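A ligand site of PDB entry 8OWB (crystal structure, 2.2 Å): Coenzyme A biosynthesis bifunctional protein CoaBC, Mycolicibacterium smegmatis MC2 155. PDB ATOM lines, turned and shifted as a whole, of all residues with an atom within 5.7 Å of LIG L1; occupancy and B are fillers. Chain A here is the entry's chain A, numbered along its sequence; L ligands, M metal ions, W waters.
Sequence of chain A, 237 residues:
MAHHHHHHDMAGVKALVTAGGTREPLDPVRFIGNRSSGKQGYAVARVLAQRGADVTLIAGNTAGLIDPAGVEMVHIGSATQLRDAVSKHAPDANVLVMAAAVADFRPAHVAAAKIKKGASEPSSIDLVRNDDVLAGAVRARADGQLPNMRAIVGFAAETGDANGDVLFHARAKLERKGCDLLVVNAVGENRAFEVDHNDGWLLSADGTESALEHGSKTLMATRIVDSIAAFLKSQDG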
ATOM      1  N   ALA A  19     -15.359 -24.367   7.409  1.00  0.00           N
ATOM      2  CA  ALA A  19     -14.705 -23.931   8.634  1.00  0.00           C
ATOM      3  C   ALA A  19     -15.110 -24.859   9.787  1.00  0.00           C
ATOM      4  O   ALA A  19     -16.170 -25.487   9.748  1.00  0.00           O
ATOM      5  CB  ALA A  19     -15.030 -22.475   8.977  1.00  0.00           C
ATOM      6  N   GLY A  20     -14.249 -24.935  10.805  1.00  0.00           N
ATOM      7  CA  GLY A  20     -14.482 -25.823  11.919  1.00  0.00           C
ATOM      8  C   GLY A  20     -13.857 -27.192  11.681  1.00  0.00           C
ATOM      9  O   GLY A  20     -13.342 -27.502  10.607  1.00  0.00           O
ATOM     10  N   SER A  36      -9.778 -27.816  16.246  1.00  0.00           N
ATOM     11  CA  SER A  36      -9.980 -26.593  15.465  1.00  0.00           C
ATOM     12  C   SER A  36     -11.205 -25.803  15.910  1.00  0.00           C
ATOM     13  O   SER A  36     -12.306 -26.358  16.013  1.00  0.00           O
ATOM     14  CB  SER A  36     -10.106 -26.958  13.993  1.00  0.00           C
ATOM     15  OG  SER A  36     -10.393 -25.816  13.207  1.00  0.00           O
ATOM     16  N   SER A  37     -11.031 -24.490  16.122  1.00  0.00           N
ATOM     17  CA  SER A  37     -12.119 -23.634  16.589  1.00  0.00           C
ATOM     18  C   SER A  37     -13.013 -23.107  15.480  1.00  0.00           C
ATOM     19  O   SER A  37     -14.148 -22.714  15.757  1.00  0.00           O
ATOM     20  CB  SER A  37     -11.556 -22.416  17.314  1.00  0.00           C
ATOM     21  OG  SER A  37     -10.987 -21.523  16.368  1.00  0.00           O
ATOM     22  N   GLY A  38     -12.528 -23.078  14.238  1.00  0.00           N
ATOM     23  CA  GLY A  38     -13.288 -22.513  13.143  1.00  0.00           C
ATOM     24  C   GLY A  38     -13.288 -21.000  13.049  1.00  0.00           C
ATOM     25  O   GLY A  38     -13.845 -20.463  12.101  1.00  0.00           O
ATOM     26  N   LYS A  39     -12.633 -20.296  13.974  1.00  0.00           N
ATOM     27  CA  LYS A  39     -12.772 -18.845  14.012  1.00  0.00           C
ATOM     28  C   LYS A  39     -12.212 -18.190  12.757  1.00  0.00           C
ATOM     29  O   LYS A  39     -12.750 -17.173  12.292  1.00  0.00           O
ATOM     30  CB  LYS A  39     -12.071 -18.276  15.243  1.00  0.00           C
ATOM     31  CG  LYS A  39     -12.696 -18.659  16.573  1.00  0.00           C
ATOM     32  CD  LYS A  39     -11.947 -18.032  17.745  1.00  0.00           C
ATOM     33  N   GLN A  40     -11.181 -18.761  12.151  1.00  0.00           N
ATOM     34  CA  GLN A  40     -10.543 -18.085  11.020  1.00  0.00           C
ATOM     35  C   GLN A  40     -11.325 -18.261   9.719  1.00  0.00           C
ATOM     36  O   GLN A  40     -11.351 -17.345   8.894  1.00  0.00           O
ATOM     37  CB  GLN A  40      -9.094 -18.557  10.885  1.00  0.00           C
ATOM     38  CG  GLN A  40      -8.244 -17.746   9.918  1.00  0.00           C
ATOM     39  CD  GLN A  40      -8.034 -16.290  10.354  1.00  0.00           C
ATOM     40  OE1 GLN A  40      -7.077 -15.973  11.061  1.00  0.00           O
ATOM     41  NE2 GLN A  40      -8.922 -15.408   9.914  1.00  0.00           N
ATOM     42  N   GLY A  41     -11.953 -19.407   9.516  1.00  0.00           N
ATOM     43  CA  GLY A  41     -12.819 -19.562   8.347  1.00  0.00           C
ATOM     44  C   GLY A  41     -14.075 -18.709   8.415  1.00  0.00           C
ATOM     45  O   GLY A  41     -14.500 -18.132   7.405  1.00  0.00           O
ATOM     46  N   MET A  98     -10.964 -23.760   1.776  1.00  0.00           N
ATOM     47  CA  MET A  98     -11.080 -24.965   2.573  1.00  0.00           C
ATOM     48  C   MET A  98     -10.419 -24.736   3.916  1.00  0.00           C
ATOM     49  O   MET A  98      -9.318 -25.215   4.184  1.00  0.00           O
ATOM     50  CB  MET A  98     -10.456 -26.156   1.833  1.00  0.00           C
ATOM     51  CG  MET A  98     -11.328 -26.678   0.715  1.00  0.00           C
ATOM     52  SD  MET A  98     -12.859 -27.478   1.243  1.00  0.00           S
ATOM     53  CE  MET A  98     -12.315 -28.895   2.191  1.00  0.00           C
ATOM     54  N   ALA A  99     -11.112 -24.033   4.805  1.00  0.00           N
ATOM     55  CA  ALA A  99     -10.514 -23.742   6.101  1.00  0.00           C
ATOM     56  C   ALA A  99     -10.899 -24.741   7.196  1.00  0.00           C
ATOM     57  O   ALA A  99     -10.523 -24.531   8.350  1.00  0.00           O
ATOM     58  CB  ALA A  99     -10.891 -22.326   6.552  1.00  0.00           C
ATOM     59  N   ALA A 100     -11.658 -25.784   6.869  1.00  0.00           N
ATOM     60  CA  ALA A 100     -12.074 -26.766   7.856  1.00  0.00           C
ATOM     61  C   ALA A 100     -10.955 -27.745   8.164  1.00  0.00           C
ATOM     62  O   ALA A 100     -10.180 -28.138   7.289  1.00  0.00           O
ATOM     63  CB  ALA A 100     -13.297 -27.538   7.382  1.00  0.00           C
ATOM     64  N   ALA A 101     -10.897 -28.177   9.429  1.00  0.00           N
ATOM     65  CA  ALA A 101      -9.996 -29.253   9.835  1.00  0.00           C
ATOM     66  C   ALA A 101     -10.697 -30.568   9.519  1.00  0.00           C
ATOM     67  O   ALA A 101     -11.403 -31.147  10.349  1.00  0.00           O
ATOM     68  CB  ALA A 101      -9.654 -29.130  11.306  1.00  0.00           C
ATOM     69  N   VAL A 102     -10.566 -31.005   8.278  1.00  0.00           N
ATOM     70  CA  VAL A 102     -11.234 -32.223   7.850  1.00  0.00           C
ATOM     71  C   VAL A 102     -10.474 -33.420   8.384  1.00  0.00           C
ATOM     72  O   VAL A 102      -9.256 -33.529   8.181  1.00  0.00           O
ATOM     73  CB  VAL A 102     -11.366 -32.271   6.313  1.00  0.00           C
ATOM     74  CG1 VAL A 102     -12.214 -33.456   5.910  1.00  0.00           C
ATOM     75  CG2 VAL A 102     -11.971 -30.962   5.774  1.00  0.00           C
ATOM     76  N   PHE A 155      -5.835 -24.524   3.524  1.00  0.00           N
ATOM     77  CA  PHE A 155      -5.310 -24.064   4.807  1.00  0.00           C
ATOM     78  C   PHE A 155      -4.415 -25.136   5.390  1.00  0.00           C
ATOM     79  O   PHE A 155      -4.605 -26.312   5.133  1.00  0.00           O
ATOM     80  CB  PHE A 155      -6.420 -23.767   5.786  1.00  0.00           C
ATOM     81  CG  PHE A 155      -6.938 -22.380   5.690  1.00  0.00           C
ATOM     82  CD1 PHE A 155      -7.377 -21.874   4.476  1.00  0.00           C
ATOM     83  CD2 PHE A 155      -7.031 -21.585   6.806  1.00  0.00           C
ATOM     84  CE1 PHE A 155      -7.870 -20.595   4.385  1.00  0.00           C
ATOM     85  CE2 PHE A 155      -7.546 -20.303   6.724  1.00  0.00           C
ATOM     86  CZ  PHE A 155      -7.957 -19.801   5.514  1.00  0.00           C
ATOM     87  N   ALA A 156      -3.394 -24.706   6.119  1.00  0.00           N
ATOM     88  CA  ALA A 156      -2.505 -25.662   6.759  1.00  0.00           C
ATOM     89  C   ALA A 156      -1.837 -25.011   7.963  1.00  0.00           C
ATOM     90  O   ALA A 156      -1.592 -23.799   7.997  1.00  0.00           O
ATOM     91  CB  ALA A 156      -1.458 -26.194   5.771  1.00  0.00           C
ATOM     92  N   ALA A 157      -1.582 -25.831   8.981  1.00  0.00           N
ATOM     93  CA  ALA A 157      -0.744 -25.468  10.115  1.00  0.00           C
ATOM     94  C   ALA A 157       0.471 -26.374  10.075  1.00  0.00           C
ATOM     95  O   ALA A 157       0.347 -27.584  10.237  1.00  0.00           O
ATOM     96  CB  ALA A 157      -1.495 -25.634  11.440  1.00  0.00           C
ATOM     97  N   VAL A 183      -2.982 -20.928   2.747  1.00  0.00           N
ATOM     98  CA  VAL A 183      -2.879 -20.070   3.923  1.00  0.00           C
ATOM     99  C   VAL A 183      -2.273 -20.904   5.050  1.00  0.00           C
ATOM    100  O   VAL A 183      -2.932 -21.777   5.621  1.00  0.00           O
ATOM    101  CB  VAL A 183      -4.225 -19.466   4.317  1.00  0.00           C
ATOM    102  CG1 VAL A 183      -4.030 -18.515   5.457  1.00  0.00           C
ATOM    103  CG2 VAL A 183      -4.811 -18.739   3.144  1.00  0.00           C
ATOM    104  N   VAL A 184      -1.009 -20.660   5.347  1.00  0.00           N
ATOM    105  CA  VAL A 184      -0.236 -21.480   6.253  1.00  0.00           C
ATOM    106  C   VAL A 184      -0.057 -20.776   7.578  1.00  0.00           C
ATOM    107  O   VAL A 184       0.442 -19.643   7.624  1.00  0.00           O
ATOM    108  CB  VAL A 184       1.128 -21.821   5.636  1.00  0.00           C
ATOM    109  CG1 VAL A 184       1.910 -22.713   6.556  1.00  0.00           C
ATOM    110  CG2 VAL A 184       0.929 -22.434   4.257  1.00  0.00           C
ATOM    111  N   ASN A 185      -0.405 -21.442   8.668  1.00  0.00           N
ATOM    112  CA  ASN A 185      -0.072 -20.989  10.008  1.00  0.00           C
ATOM    113  C   ASN A 185       1.183 -21.717  10.480  1.00  0.00           C
ATOM    114  O   ASN A 185       1.295 -22.940  10.333  1.00  0.00           O
ATOM    115  CB  ASN A 185      -1.220 -21.230  10.985  1.00  0.00           C
ATOM    116  CG  ASN A 185      -0.850 -20.871  12.417  1.00  0.00           C
ATOM    117  OD1 ASN A 185      -0.625 -19.708  12.751  1.00  0.00           O
ATOM    118  ND2 ASN A 185      -0.779 -21.877  13.279  1.00  0.00           N
ATOM    119  N   ASP A 199       2.185 -15.842  13.320  1.00  0.00           N
ATOM    120  CA  ASP A 199       2.211 -15.606  11.888  1.00  0.00           C
ATOM    121  C   ASP A 199       2.137 -16.818  11.009  1.00  0.00           C
ATOM    122  O   ASP A 199       1.655 -17.861  11.395  1.00  0.00           O
ATOM    123  CB  ASP A 199       3.580 -15.011  11.498  1.00  0.00           C
ATOM    124  CG  ASP A 199       3.970 -13.768  12.245  1.00  0.00           C
ATOM    125  OD1 ASP A 199       4.564 -12.889  11.584  1.00  0.00           O
ATOM    126  OD2 ASP A 199       3.748 -13.650  13.474  1.00  0.00           O
ATOM    127  N   LEU A 212       2.459 -13.787   6.669  1.00  0.00           N
ATOM    128  CA  LEU A 212       1.122 -13.519   7.179  1.00  0.00           C
ATOM    129  C   LEU A 212       1.340 -12.838   8.511  1.00  0.00           C
ATOM    130  O   LEU A 212       1.669 -13.488   9.506  1.00  0.00           O
ATOM    131  CB  LEU A 212       0.317 -14.802   7.321  1.00  0.00           C
ATOM    132  CG  LEU A 212      -1.131 -14.544   7.706  1.00  0.00           C
ATOM    133  CD1 LEU A 212      -1.657 -13.326   6.948  1.00  0.00           C
ATOM    134  CD2 LEU A 212      -1.958 -15.793   7.427  1.00  0.00           C
ATOM    135  N   LYS A 217      -8.453 -12.478  14.187  1.00  0.00           N
ATOM    136  CA  LYS A 217      -9.005 -13.312  13.122  1.00  0.00           C
ATOM    137  C   LYS A 217      -9.570 -12.432  12.013  1.00  0.00           C
ATOM    138  O   LYS A 217      -9.446 -12.758  10.837  1.00  0.00           O
ATOM    139  CB  LYS A 217     -10.076 -14.246  13.678  1.00  0.00           C
ATOM    140  CG  LYS A 217      -9.585 -15.277  14.698  1.00  0.00           C
ATOM    141  CD  LYS A 217      -8.484 -16.198  14.176  1.00  0.00           C
ATOM    142  CE  LYS A 217      -7.929 -17.071  15.312  1.00  0.00           C
ATOM    143  NZ  LYS A 217      -6.690 -17.788  14.934  1.00  0.00           N
ATOM    144  N   MET A 220      -6.531 -10.746   9.920  1.00  0.00           N
ATOM    145  CA  MET A 220      -5.858 -11.750   9.099  1.00  0.00           C
ATOM    146  C   MET A 220      -6.775 -12.230   7.986  1.00  0.00           C
ATOM    147  O   MET A 220      -6.321 -12.508   6.870  1.00  0.00           O
ATOM    148  CB  MET A 220      -5.369 -12.895   9.975  1.00  0.00           C
ATOM    149  CG  MET A 220      -4.122 -12.470  10.785  1.00  0.00           C
ATOM    150  SD  MET A 220      -3.223 -13.810  11.582  1.00  0.00           S
ATOM    151  CE  MET A 220      -4.405 -14.429  12.771  1.00  0.00           C
ATOM    152  N   ILE A 224      -6.137 -12.376   3.938  1.00  0.00           N
ATOM    153  CA  ILE A 224      -6.436 -13.537   3.110  1.00  0.00           C
ATOM    154  C   ILE A 224      -7.301 -13.137   1.920  1.00  0.00           C
ATOM    155  O   ILE A 224      -7.028 -13.492   0.776  1.00  0.00           O
ATOM    156  CB  ILE A 224      -7.093 -14.644   3.944  1.00  0.00           C
ATOM    157  CG1 ILE A 224      -6.093 -15.167   4.982  1.00  0.00           C
ATOM    158  CG2 ILE A 224      -7.570 -15.760   3.050  1.00  0.00           C
ATOM    159  CD1 ILE A 224      -6.730 -15.920   6.123  1.00  0.00           C
HETATM  160  N1  LIG L   1      -6.414 -23.691  10.321  1.00  0.00           N
HETATM  161  C1  LIG L   1      -6.323 -24.992   9.774  1.00  0.00           C
HETATM  162  C2  LIG L   1      -5.097 -27.003   9.330  1.00  0.00           C
HETATM  163  C3  LIG L   1      -5.680 -22.623  10.008  1.00  0.00           C
HETATM  164  C4  LIG L   1      -4.628 -22.421   9.102  1.00  0.00           C
HETATM  165  C5  LIG L   1      -4.043 -21.164   8.996  1.00  0.00           C
HETATM  166  C6  LIG L   1      -4.484 -20.095   9.786  1.00  0.00           C
HETATM  167  C7  LIG L   1      -5.512 -20.289  10.691  1.00  0.00           C
HETATM  168  C8  LIG L   1      -6.105 -21.550  10.793  1.00  0.00           C
HETATM  169  C9  LIG L   1      -7.175 -22.057  11.615  1.00  0.00           C
HETATM  170  C10 LIG L   1      -7.968 -21.260  12.632  1.00  0.00           C
HETATM  171  C11 LIG L   1      -9.484 -21.339  12.798  1.00  0.00           C
HETATM  172  C12 LIG L   1      -7.308 -23.398  11.256  1.00  0.00           C
HETATM  173  C13 LIG L   1      -5.149 -25.737   9.875  1.00  0.00           C
HETATM  174  C14 LIG L   1      -6.197 -27.533   8.684  1.00  0.00           C
HETATM  175  C15 LIG L   1      -7.358 -26.803   8.578  1.00  0.00           C
HETATM  176  C16 LIG L   1      -7.417 -25.530   9.125  1.00  0.00           C
HETATM  177  O1  LIG L   1      -9.945 -21.184  13.976  1.00  0.00           O
HETATM  178  O2  LIG L   1     -10.269 -21.561  11.828  1.00  0.00           O
HETATM  179  O3  LIG L   1      -7.371 -20.504  13.379  1.00  0.00           O
HETATM  180  O4  LIG L   1      -6.129 -28.831   8.146  1.00  0.00           O
HETATM  181 BR1  LIG L   1      -3.670 -18.352   9.622  1.00  0.00          BR
HETATM  182  N1  LG2 L   2      -8.602 -31.348   3.805  1.00  0.00           N
HETATM  183  C1  LG2 L   2      -9.557 -31.886   2.967  1.00  0.00           C
HETATM  184  N2  LG2 L   2      -9.954 -33.195   3.112  1.00  0.00           N
HETATM  185  C2  LG2 L   2      -9.272 -34.030   3.983  1.00  0.00           C
HETATM  186  C3  LG2 L   2      -8.187 -33.510   4.717  1.00  0.00           C
HETATM  187  C4  LG2 L   2      -7.813 -32.185   4.552  1.00  0.00           C
HETATM  188  O1  LG2 L   2     -10.063 -31.205   2.072  1.00  0.00           O
HETATM  189  N3  LG2 L   2      -9.668 -35.304   4.115  1.00  0.00           N
HETATM  190  C5  LG2 L   2      -8.131 -29.989   3.514  1.00  0.00           C
HETATM  191  C6  LG2 L   2      -8.218 -29.068   4.721  1.00  0.00           C
HETATM  192  O2  LG2 L   2      -9.408 -28.334   4.709  1.00  0.00           O
HETATM  193  C7  LG2 L   2      -7.052 -28.147   4.507  1.00  0.00           C
HETATM  194  C8  LG2 L   2      -6.105 -28.882   3.587  1.00  0.00           C
HETATM  195  O3  LG2 L   2      -6.773 -30.029   3.134  1.00  0.00           O
HETATM  196  O4  LG2 L   2      -7.499 -27.012   3.812  1.00  0.00           O
HETATM  197  C9  LG2 L   2      -4.831 -29.359   4.268  1.00  0.00           C
HETATM  198  O5  LG2 L   2      -5.068 -29.997   5.508  1.00  0.00           O
HETATM  199  P1  LG2 L   2      -3.844 -30.862   6.088  1.00  0.00           P
HETATM  200  O6  LG2 L   2      -2.759 -29.935   6.571  1.00  0.00           O
HETATM  201  O7  LG2 L   2      -4.302 -31.856   7.143  1.00  0.00           O
HETATM  202  O8  LG2 L   2      -3.405 -31.624   4.737  1.00  0.00           O
HETATM  203  P2  LG2 L   2      -3.017 -33.151   4.925  1.00  0.00           P
HETATM  204  O9  LG2 L   2      -2.490 -33.834   3.691  1.00  0.00           O
HETATM  205  O10 LG2 L   2      -4.142 -33.915   5.575  1.00  0.00           O
HETATM  206  O11 LG2 L   2      -1.876 -32.885   6.022  1.00  0.00           O
HETATM  207  P3  LG2 L   2      -1.163 -34.011   6.920  1.00  0.00           P
HETATM  208  O12 LG2 L   2       0.149 -33.386   7.325  1.00  0.00           O
HETATM  209  O13 LG2 L   2      -0.935 -35.264   6.105  1.00  0.00           O
HETATM  210  O14 LG2 L   2      -2.053 -34.294   8.099  1.00  0.00           O
HETATM  211 CA    CA M   1      -4.547 -34.241   7.758  1.00  0.00          CA
HETATM  212  O   HOH W   1      -7.974 -23.487  14.942  1.00  0.00           O
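The backbone NH of Lys 39 lies within hydrogen-bond range of an oxygen (O1) of LIG L1 (2.8 Å). NZ of Lys 217 lies within hydrogen-bond range of O3 of LIG L1 (3.2 Å). N of Gly 38 sits at hydrogen-bond distance from O1 of LIG L1, at 3.2 Å. O4 of LG2 L2 lies close to O of Phe 155, at 3.3 Å. OG of Ser 37 sits at hydrogen-bond distance from O1 of LIG L1 (2.6 Å). O of Met 98 lies within hydrogen-bond range of O4 of LG2 L2, at 2.6 Å. The backbone NH (N) of Gln 40 is in hydrogen-bond range of an oxygen (O2) of LIG L1, 3.0 Å away. An oxygen (O2) of LG2 L2 sits at hydrogen-bond distance from the backbone carbonyl oxygen of Ala 100. The backbone NH of Phe 155 lies within hydrogen-bond range of an oxygen (O4) of LG2 L2 (3.0 Å).
An oxygen (O5) of LG2 L2 is in hydrogen-bond range of an oxygen (O4) of LIG L1.
O of Lys 217 lies within hydrogen-bond range of NE2 of Gln 40. O of Asp 199 sits close to OD1 of Asn 185, 3.2 Å away. The backbone carbonyl oxygen of Val 183 sits at hydrogen-bond distance from the backbone NH of Ala 156. The backbone carbonyl oxygen (O) of Gly 20 lies within hydrogen-bond range of the backbone NH (N) of Ala 101. O of Ala 156 lies within hydrogen-bond range of N of Asn 185. The side-chain hydroxyl of Ser 37 sits at hydrogen-bond distance from the backbone NH of Lys 39, 3.2 Å away.
Gly 41 touches LIG L1 (N to O2, 3.6 Å). O of Ala 99 touches C16 of LIG L1, at 3.4 Å. Ala 100 touches LIG L1. CA of Ala 101 touches C15 of LIG L1, 3.8 Å away. CD2 of Phe 155 touches C4 of LIG L1, 3.4 Å away. O of Ala 156 touches C4 of LIG L1, 3.5 Å away. Ala 157 touches LIG L1. Val 183 touches LIG L1. CB of Asn 185 touches C5 of LIG L1, 3.5 Å away. Leu 212 touches LIG L1 (CD2 to BR1, 3.8 Å). Hydrophobic or aromatic side chains within 4 Å of LIG L1: Phe 155, Ala 157 and Leu 212. Within 4 Å of LIG L1: Ser 37, Gly 38, Lys 39, Gln 40, Gly 41, Ala 99, Ala 100, Ala 101, Phe 155, Ala 156, Ala 157, Val 183, Asn 185, Leu 212 and Lys 217. The nearest printed residue that does not touch LIG L1 is Val 184 (4.2 Å).
Water W1 bridges O1 of LIG L1 (3.2 Å) and N of Ser 37 (3.4 Å).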
